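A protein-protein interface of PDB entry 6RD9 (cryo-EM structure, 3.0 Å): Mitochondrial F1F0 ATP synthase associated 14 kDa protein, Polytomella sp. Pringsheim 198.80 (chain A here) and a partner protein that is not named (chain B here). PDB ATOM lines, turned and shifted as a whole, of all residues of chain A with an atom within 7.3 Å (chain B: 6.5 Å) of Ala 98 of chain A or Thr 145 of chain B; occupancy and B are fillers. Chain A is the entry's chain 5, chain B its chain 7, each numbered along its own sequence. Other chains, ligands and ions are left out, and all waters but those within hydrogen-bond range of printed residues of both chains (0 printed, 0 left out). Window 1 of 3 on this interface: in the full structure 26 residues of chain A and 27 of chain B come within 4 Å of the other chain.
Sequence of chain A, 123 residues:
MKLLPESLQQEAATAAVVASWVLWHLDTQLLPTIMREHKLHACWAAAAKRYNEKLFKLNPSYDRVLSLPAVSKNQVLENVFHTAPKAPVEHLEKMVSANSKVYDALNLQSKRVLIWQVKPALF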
ATOM      1  N   LEU A  92     -17.666  17.021 -32.659  1.00  0.00           N
ATOM      2  CA  LEU A  92     -18.939  17.718 -32.620  1.00  0.00           C
ATOM      3  C   LEU A  92     -19.789  17.203 -31.477  1.00  0.00           C
ATOM      4  O   LEU A  92     -20.097  17.941 -30.546  1.00  0.00           O
ATOM      5  CB  LEU A  92     -19.663  17.572 -33.955  1.00  0.00           C
ATOM      6  CG  LEU A  92     -20.924  18.398 -34.174  1.00  0.00           C
ATOM      7  CD1 LEU A  92     -20.995  18.823 -35.583  1.00  0.00           C
ATOM      8  CD2 LEU A  92     -22.149  17.598 -33.904  1.00  0.00           C
ATOM      9  N   GLU A  93     -20.119  15.918 -31.487  1.00  0.00           N
ATOM     10  CA  GLU A  93     -21.081  15.384 -30.534  1.00  0.00           C
ATOM     11  C   GLU A  93     -20.553  15.275 -29.113  1.00  0.00           C
ATOM     12  O   GLU A  93     -21.294  14.824 -28.242  1.00  0.00           O
ATOM     13  CB  GLU A  93     -21.559  14.016 -30.986  1.00  0.00           C
ATOM     14  CG  GLU A  93     -20.495  12.967 -30.987  1.00  0.00           C
ATOM     15  CD  GLU A  93     -21.064  11.578 -31.176  1.00  0.00           C
ATOM     16  OE1 GLU A  93     -22.294  11.433 -31.048  1.00  0.00           O
ATOM     17  OE2 GLU A  93     -20.291  10.637 -31.453  1.00  0.00           O
ATOM     18  N   LYS A  94     -19.308  15.654 -28.861  1.00  0.00           N
ATOM     19  CA  LYS A  94     -18.764  15.725 -27.518  1.00  0.00           C
ATOM     20  C   LYS A  94     -18.672  17.141 -27.007  1.00  0.00           C
ATOM     21  O   LYS A  94     -18.780  17.357 -25.804  1.00  0.00           O
ATOM     22  CB  LYS A  94     -17.378  15.092 -27.483  1.00  0.00           C
ATOM     23  CG  LYS A  94     -17.315  13.654 -27.828  1.00  0.00           C
ATOM     24  CD  LYS A  94     -15.926  13.133 -27.690  1.00  0.00           C
ATOM     25  CE  LYS A  94     -15.548  13.053 -26.243  1.00  0.00           C
ATOM     26  NZ  LYS A  94     -16.330  12.012 -25.531  1.00  0.00           N
ATOM     27  N   MET A  95     -18.468  18.112 -27.894  1.00  0.00           N
ATOM     28  CA  MET A  95     -18.531  19.507 -27.496  1.00  0.00           C
ATOM     29  C   MET A  95     -19.953  20.018 -27.488  1.00  0.00           C
ATOM     30  O   MET A  95     -20.258  20.953 -26.755  1.00  0.00           O
ATOM     31  CB  MET A  95     -17.704  20.369 -28.426  1.00  0.00           C
ATOM     32  CG  MET A  95     -16.258  20.073 -28.405  1.00  0.00           C
ATOM     33  SD  MET A  95     -15.441  20.368 -26.859  1.00  0.00           S
ATOM     34  CE  MET A  95     -15.013  22.070 -27.068  1.00  0.00           C
ATOM     35  N   VAL A  96     -20.829  19.444 -28.306  1.00  0.00           N
ATOM     36  CA  VAL A  96     -22.216  19.884 -28.336  1.00  0.00           C
ATOM     37  C   VAL A  96     -22.931  19.484 -27.060  1.00  0.00           C
ATOM     38  O   VAL A  96     -23.650  20.287 -26.461  1.00  0.00           O
ATOM     39  CB  VAL A  96     -22.912  19.336 -29.589  1.00  0.00           C
ATOM     40  CG1 VAL A  96     -24.394  19.352 -29.435  1.00  0.00           C
ATOM     41  CG2 VAL A  96     -22.534  20.175 -30.758  1.00  0.00           C
ATOM     42  N   SER A  97     -22.706  18.263 -26.592  1.00  0.00           N
ATOM     43  CA  SER A  97     -23.274  17.834 -25.325  1.00  0.00           C
ATOM     44  C   SER A  97     -22.687  18.573 -24.139  1.00  0.00           C
ATOM     45  O   SER A  97     -23.313  18.610 -23.082  1.00  0.00           O
ATOM     46  CB  SER A  97     -23.052  16.351 -25.121  1.00  0.00           C
ATOM     47  OG  SER A  97     -21.703  16.115 -24.797  1.00  0.00           O
ATOM     48  N   ALA A  98     -21.502  19.143 -24.278  1.00  0.00           N
ATOM     49  CA  ALA A  98     -20.928  19.943 -23.218  1.00  0.00           C
ATOM     50  C   ALA A  98     -21.314  21.397 -23.325  1.00  0.00           C
ATOM     51  O   ALA A  98     -21.340  22.090 -22.315  1.00  0.00           O
ATOM     52  CB  ALA A  98     -19.411  19.827 -23.221  1.00  0.00           C
ATOM     53  N   ASN A  99     -21.588  21.890 -24.521  1.00  0.00           N
ATOM     54  CA  ASN A  99     -22.141  23.221 -24.652  1.00  0.00           C
ATOM     55  C   ASN A  99     -23.635  23.250 -24.426  1.00  0.00           C
ATOM     56  O   ASN A  99     -24.195  24.327 -24.252  1.00  0.00           O
ATOM     57  CB  ASN A  99     -21.844  23.796 -26.019  1.00  0.00           C
ATOM     58  CG  ASN A  99     -20.403  24.024 -26.243  1.00  0.00           C
ATOM     59  OD1 ASN A  99     -19.631  24.092 -25.310  1.00  0.00           O
ATOM     60  ND2 ASN A  99     -20.018  24.150 -27.492  1.00  0.00           N
ATOM     61  N   SER A 100     -24.301  22.104 -24.427  1.00  0.00           N
ATOM     62  CA  SER A 100     -25.693  22.086 -24.023  1.00  0.00           C
ATOM     63  C   SER A 100     -25.842  22.303 -22.533  1.00  0.00           C
ATOM     64  O   SER A 100     -26.939  22.604 -22.074  1.00  0.00           O
ATOM     65  CB  SER A 100     -26.353  20.773 -24.395  1.00  0.00           C
ATOM     66  OG  SER A 100     -25.897  19.735 -23.564  1.00  0.00           O
ATOM     67  N   LYS A 101     -24.777  22.106 -21.765  1.00  0.00           N
ATOM     68  CA  LYS A 101     -24.755  22.495 -20.369  1.00  0.00           C
ATOM     69  C   LYS A 101     -24.370  23.952 -20.191  1.00  0.00           C
ATOM     70  O   LYS A 101     -24.724  24.556 -19.184  1.00  0.00           O
ATOM     71  CB  LYS A 101     -23.791  21.603 -19.616  1.00  0.00           C
ATOM     72  CG  LYS A 101     -24.309  20.221 -19.382  1.00  0.00           C
ATOM     73  CD  LYS A 101     -23.242  19.203 -19.555  1.00  0.00           C
ATOM     74  CE  LYS A 101     -22.065  19.480 -18.690  1.00  0.00           C
ATOM     75  NZ  LYS A 101     -21.074  18.408 -18.778  1.00  0.00           N
ATOM     76  N   VAL A 102     -23.626  24.523 -21.130  1.00  0.00           N
ATOM     77  CA  VAL A 102     -23.405  25.962 -21.154  1.00  0.00           C
ATOM     78  C   VAL A 102     -24.670  26.686 -21.576  1.00  0.00           C
ATOM     79  O   VAL A 102     -24.927  27.809 -21.146  1.00  0.00           O
ATOM     80  CB  VAL A 102     -22.226  26.287 -22.081  1.00  0.00           C
ATOM     81  CG1 VAL A 102     -21.862  27.715 -22.042  1.00  0.00           C
ATOM     82  CG2 VAL A 102     -21.060  25.522 -21.665  1.00  0.00           C
ATOM     83  N   TYR A 103     -25.477  26.071 -22.431  1.00  0.00           N
ATOM     84  CA  TYR A 103     -26.752  26.687 -22.761  1.00  0.00           C
ATOM     85  C   TYR A 103     -27.680  26.646 -21.576  1.00  0.00           C
ATOM     86  O   TYR A 103     -28.359  27.632 -21.301  1.00  0.00           O
ATOM     87  CB  TYR A 103     -27.432  25.999 -23.941  1.00  0.00           C
ATOM     88  CG  TYR A 103     -28.796  26.574 -24.258  1.00  0.00           C
ATOM     89  CD1 TYR A 103     -28.920  27.732 -24.969  1.00  0.00           C
ATOM     90  CD2 TYR A 103     -29.959  25.958 -23.830  1.00  0.00           C
ATOM     91  CE1 TYR A 103     -30.129  28.249 -25.254  1.00  0.00           C
ATOM     92  CE2 TYR A 103     -31.171  26.500 -24.090  1.00  0.00           C
ATOM     93  CZ  TYR A 103     -31.246  27.638 -24.807  1.00  0.00           C
ATOM     94  OH  TYR A 103     -32.458  28.185 -25.088  1.00  0.00           O
ATOM     95  N   ALA A 105     -27.229  26.367 -18.236  1.00  0.00           N
ATOM     96  CA  ALA A 105     -26.956  27.154 -17.061  1.00  0.00           C
ATOM     97  C   ALA A 105     -26.901  28.637 -17.352  1.00  0.00           C
ATOM     98  O   ALA A 105     -27.168  29.433 -16.459  1.00  0.00           O
ATOM     99  CB  ALA A 105     -25.658  26.700 -16.448  1.00  0.00           C
ATOM    100  N   LEU A 106     -26.581  29.049 -18.568  1.00  0.00           N
ATOM    101  CA  LEU A 106     -26.101  30.411 -18.726  1.00  0.00           C
ATOM    102  C   LEU A 106     -26.771  31.156 -19.860  1.00  0.00           C
ATOM    103  O   LEU A 106     -26.147  32.015 -20.481  1.00  0.00           O
ATOM    104  CB  LEU A 106     -24.608  30.428 -18.994  1.00  0.00           C
ATOM    105  CG  LEU A 106     -23.632  29.730 -18.088  1.00  0.00           C
ATOM    106  CD1 LEU A 106     -22.371  29.656 -18.837  1.00  0.00           C
ATOM    107  CD2 LEU A 106     -23.431  30.522 -16.863  1.00  0.00           C
ATOM    108  N   TYR B 101     -12.665  28.154 -17.372  1.00  0.00           N
ATOM    109  CA  TYR B 101     -13.192  28.049 -18.716  1.00  0.00           C
ATOM    110  C   TYR B 101     -12.476  28.983 -19.673  1.00  0.00           C
ATOM    111  O   TYR B 101     -12.454  28.726 -20.872  1.00  0.00           O
ATOM    112  CB  TYR B 101     -14.676  28.365 -18.658  1.00  0.00           C
ATOM    113  CG  TYR B 101     -15.459  28.359 -19.927  1.00  0.00           C
ATOM    114  CD1 TYR B 101     -16.184  27.257 -20.297  1.00  0.00           C
ATOM    115  CD2 TYR B 101     -15.546  29.489 -20.710  1.00  0.00           C
ATOM    116  CE1 TYR B 101     -16.921  27.274 -21.424  1.00  0.00           C
ATOM    117  CE2 TYR B 101     -16.256  29.491 -21.840  1.00  0.00           C
ATOM    118  CZ  TYR B 101     -16.945  28.393 -22.183  1.00  0.00           C
ATOM    119  OH  TYR B 101     -17.674  28.439 -23.317  1.00  0.00           O
ATOM    120  N   TYR B 138     -11.498  16.821 -23.423  1.00  0.00           N
ATOM    121  CA  TYR B 138     -12.911  16.564 -23.238  1.00  0.00           C
ATOM    122  C   TYR B 138     -13.210  16.150 -21.817  1.00  0.00           C
ATOM    123  O   TYR B 138     -14.348  16.254 -21.381  1.00  0.00           O
ATOM    124  CB  TYR B 138     -13.389  15.492 -24.198  1.00  0.00           C
ATOM    125  CG  TYR B 138     -13.199  15.857 -25.629  1.00  0.00           C
ATOM    126  CD1 TYR B 138     -13.508  17.113 -26.084  1.00  0.00           C
ATOM    127  CD2 TYR B 138     -12.703  14.946 -26.525  1.00  0.00           C
ATOM    128  CE1 TYR B 138     -13.335  17.442 -27.389  1.00  0.00           C
ATOM    129  CE2 TYR B 138     -12.523  15.272 -27.827  1.00  0.00           C
ATOM    130  CZ  TYR B 138     -12.837  16.519 -28.248  1.00  0.00           C
ATOM    131  OH  TYR B 138     -12.653  16.843 -29.556  1.00  0.00           O
ATOM    132  N   LEU B 140     -11.597  17.651 -19.228  1.00  0.00           N
ATOM    133  CA  LEU B 140     -11.539  18.919 -18.523  1.00  0.00           C
ATOM    134  C   LEU B 140     -12.699  19.809 -18.905  1.00  0.00           C
ATOM    135  O   LEU B 140     -13.239  20.516 -18.062  1.00  0.00           O
ATOM    136  CB  LEU B 140     -10.237  19.640 -18.831  1.00  0.00           C
ATOM    137  CG  LEU B 140      -8.930  18.918 -18.609  1.00  0.00           C
ATOM    138  CD1 LEU B 140      -7.799  19.798 -19.025  1.00  0.00           C
ATOM    139  CD2 LEU B 140      -8.823  18.529 -17.188  1.00  0.00           C
ATOM    140  N   TYR B 141     -13.092  19.798 -20.166  1.00  0.00           N
ATOM    141  CA  TYR B 141     -14.143  20.688 -20.615  1.00  0.00           C
ATOM    142  C   TYR B 141     -15.520  20.215 -20.209  1.00  0.00           C
ATOM    143  O   TYR B 141     -16.401  21.037 -19.985  1.00  0.00           O
ATOM    144  CB  TYR B 141     -14.082  20.838 -22.119  1.00  0.00           C
ATOM    145  CG  TYR B 141     -15.001  21.867 -22.664  1.00  0.00           C
ATOM    146  CD1 TYR B 141     -14.706  23.199 -22.563  1.00  0.00           C
ATOM    147  CD2 TYR B 141     -16.163  21.504 -23.296  1.00  0.00           C
ATOM    148  CE1 TYR B 141     -15.541  24.131 -23.068  1.00  0.00           C
ATOM    149  CE2 TYR B 141     -17.000  22.437 -23.802  1.00  0.00           C
ATOM    150  CZ  TYR B 141     -16.685  23.740 -23.684  1.00  0.00           C
ATOM    151  OH  TYR B 141     -17.539  24.665 -24.191  1.00  0.00           O
ATOM    152  N   GLU B 142     -15.747  18.918 -20.115  1.00  0.00           N
ATOM    153  CA  GLU B 142     -17.065  18.465 -19.714  1.00  0.00           C
ATOM    154  C   GLU B 142     -17.293  18.586 -18.227  1.00  0.00           C
ATOM    155  O   GLU B 142     -18.431  18.458 -17.790  1.00  0.00           O
ATOM    156  CB  GLU B 142     -17.305  17.025 -20.159  1.00  0.00           C
ATOM    157  CG  GLU B 142     -17.450  16.877 -21.666  1.00  0.00           C
ATOM    158  CD  GLU B 142     -17.909  15.502 -22.093  1.00  0.00           C
ATOM    159  OE1 GLU B 142     -17.450  14.506 -21.489  1.00  0.00           O
ATOM    160  OE2 GLU B 142     -18.716  15.418 -23.046  1.00  0.00           O
ATOM    161  N   THR B 143     -16.254  18.808 -17.437  1.00  0.00           N
ATOM    162  CA  THR B 143     -16.444  19.030 -16.018  1.00  0.00           C
ATOM    163  C   THR B 143     -16.395  20.491 -15.626  1.00  0.00           C
ATOM    164  O   THR B 143     -16.894  20.832 -14.560  1.00  0.00           O
ATOM    165  CB  THR B 143     -15.417  18.258 -15.186  1.00  0.00           C
ATOM    166  OG1 THR B 143     -15.676  18.503 -13.812  1.00  0.00           O
ATOM    167  CG2 THR B 143     -14.057  18.717 -15.446  1.00  0.00           C
ATOM    168  N   VAL B 144     -15.833  21.372 -16.445  1.00  0.00           N
ATOM    169  CA  VAL B 144     -15.867  22.777 -16.091  1.00  0.00           C
ATOM    170  C   VAL B 144     -17.195  23.383 -16.502  1.00  0.00           C
ATOM    171  O   VAL B 144     -17.575  24.436 -15.981  1.00  0.00           O
ATOM    172  CB  VAL B 144     -14.693  23.553 -16.708  1.00  0.00           C
ATOM    173  CG1 VAL B 144     -14.966  23.924 -18.106  1.00  0.00           C
ATOM    174  CG2 VAL B 144     -14.366  24.758 -15.909  1.00  0.00           C
ATOM    175  N   THR B 145     -17.933  22.726 -17.386  1.00  0.00           N
ATOM    176  CA  THR B 145     -19.245  23.169 -17.791  1.00  0.00           C
ATOM    177  C   THR B 145     -20.328  22.403 -17.079  1.00  0.00           C
ATOM    178  O   THR B 145     -21.492  22.524 -17.430  1.00  0.00           O
ATOM    179  CB  THR B 145     -19.401  23.052 -19.292  1.00  0.00           C
ATOM    180  OG1 THR B 145     -19.286  21.688 -19.666  1.00  0.00           O
ATOM    181  CG2 THR B 145     -18.317  23.796 -19.953  1.00  0.00           C
ATOM    182  N   GLU B 146     -19.971  21.637 -16.066  1.00  0.00           N
ATOM    183  CA  GLU B 146     -20.935  21.016 -15.175  1.00  0.00           C
ATOM    184  C   GLU B 146     -21.287  22.043 -14.106  1.00  0.00           C
ATOM    185  O   GLU B 146     -20.833  21.989 -12.965  1.00  0.00           O
ATOM    186  CB  GLU B 146     -20.345  19.746 -14.590  1.00  0.00           C
ATOM    187  CG  GLU B 146     -21.258  18.903 -13.773  1.00  0.00           C
ATOM    188  CD  GLU B 146     -22.336  18.270 -14.569  1.00  0.00           C
ATOM    189  OE1 GLU B 146     -22.074  17.911 -15.727  1.00  0.00           O
ATOM    190  OE2 GLU B 146     -23.454  18.113 -14.048  1.00  0.00           O
ATOM    191  N   PHE B 147     -22.096  23.021 -14.497  1.00  0.00           N
ATOM    192  CA  PHE B 147     -22.458  24.101 -13.598  1.00  0.00           C
ATOM    193  C   PHE B 147     -23.572  23.731 -12.646  1.00  0.00           C
ATOM    194  O   PHE B 147     -23.843  24.494 -11.724  1.00  0.00           O
ATOM    195  CB  PHE B 147     -22.902  25.327 -14.370  1.00  0.00           C
ATOM    196  CG  PHE B 147     -21.908  25.834 -15.340  1.00  0.00           C
ATOM    197  CD1 PHE B 147     -20.694  26.282 -14.928  1.00  0.00           C
ATOM    198  CD2 PHE B 147     -22.212  25.895 -16.669  1.00  0.00           C
ATOM    199  CE1 PHE B 147     -19.806  26.771 -15.831  1.00  0.00           C
ATOM    200  CE2 PHE B 147     -21.333  26.387 -17.559  1.00  0.00           C
ATOM    201  CZ  PHE B 147     -20.131  26.815 -17.144  1.00  0.00           C
ATOM    202  N   ASP B 148     -24.238  22.606 -12.840  1.00  0.00           N
ATOM    203  CA  ASP B 148     -25.199  22.121 -11.869  1.00  0.00           C
ATOM    204  C   ASP B 148     -24.535  21.449 -10.689  1.00  0.00           C
ATOM    205  O   ASP B 148     -25.226  21.005  -9.774  1.00  0.00           O
ATOM    206  CB  ASP B 148     -26.164  21.142 -12.514  1.00  0.00           C
ATOM    207  CG  ASP B 148     -27.222  21.823 -13.331  1.00  0.00           C
ATOM    208  OD1 ASP B 148     -27.171  23.058 -13.469  1.00  0.00           O
ATOM    209  OD2 ASP B 148     -28.114  21.118 -13.843  1.00  0.00           O
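The backbone carbonyl oxygen (O) of Ala 98 of chain A lies within hydrogen-bond range of the side-chain hydroxyl (OG1) of Thr 145 of chain B (3.4 Å).
The side-chain hydroxyl (OH) of Tyr 141 of chain B sits at hydrogen-bond distance from the side-chain amide oxygen (OD1) of Asn 99 of chain A (2.4 Å).
NZ of Lys 101 of chain A lies within hydrogen-bond range of O of Glu 142 of chain B (2.8 Å).
OE1 of Glu 146 of chain B lies within salt-bridge range of NZ of Lys 101 of chain A.
O of Lys 94 of chain A lies close to OE2 of Glu 142 of chain B (3.4 Å).
Hydrophobic or aromatic side chains of chain A within 4 Å of the printed part of chain B: Met 95, Ala 98, Val 102, Ala 105 and Leu 106.
Among the printed residues, 16 pairs touch across the chains.
Among the printed residues, pairs that only touch across the chains: Lys 94 of chain A with Tyr 138 of chain B (3.4 Å), Met 95 of chain A with Tyr 138 of chain B (3.6 Å), Met 95 of chain A with Tyr 141 of chain B (3.8 Å), Ser 97 of chain A with Glu 142 of chain B (3.5 Å), Ala 98 of chain A with Tyr 141 of chain B (3.6 Å), Ala 98 of chain A with Glu 142 of chain B (3.9 Å), Lys 101 of chain A with Thr 145 of chain B (3.3 Å), Lys 101 of chain A with Phe 147 of chain B (3.8 Å), Val 102 of chain A with Thr 145 of chain B (3.7 Å), Ala 105 of chain A with Phe 147 of chain B (3.5 Å) and Leu 106 of chain A with Phe 147 of chain B (3.7 Å).
Of chain B, only Tyr 141 (3.6 Å), Glu 142 (3.9 Å) and Thr 145 (3.4 Å) come within 4 Å of Ala 98 of chain A.
Printed residues of chain A within 4 Å of Tyr 141 of chain B: Met 95, Ala 98 and Asn 99.
Of the printed residues of chain A, Glu 146 of chain B touches Lys 101.
The nearest residue of chain A that does not touch Thr 145 of chain B is Asn 99 of chain A (5.4 Å).
The nearest printed residue of chain B that does not touch Leu 106 of chain A is Tyr 101 of chain B (6.5 Å).
The backbone carbonyl oxygen (O) of Lys 94 of chain A is in hydrogen-bond range of the side-chain hydroxyl (OG) of Ser 97 of chain A (3.3 Å).
The backbone carbonyl oxygen (O) of Met 95 of chain A sits close to the side-chain amide nitrogen (ND2) of Asn 99 of chain A.
O of Ser 97 of chain A sits at hydrogen-bond distance from OG of Ser 100 of chain A.
The backbone carbonyl oxygen (O) of Tyr 141 of chain B lies within hydrogen-bond range of the side-chain hydroxyl (OG1) of Thr 145 of chain B, 3.0 Å away.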
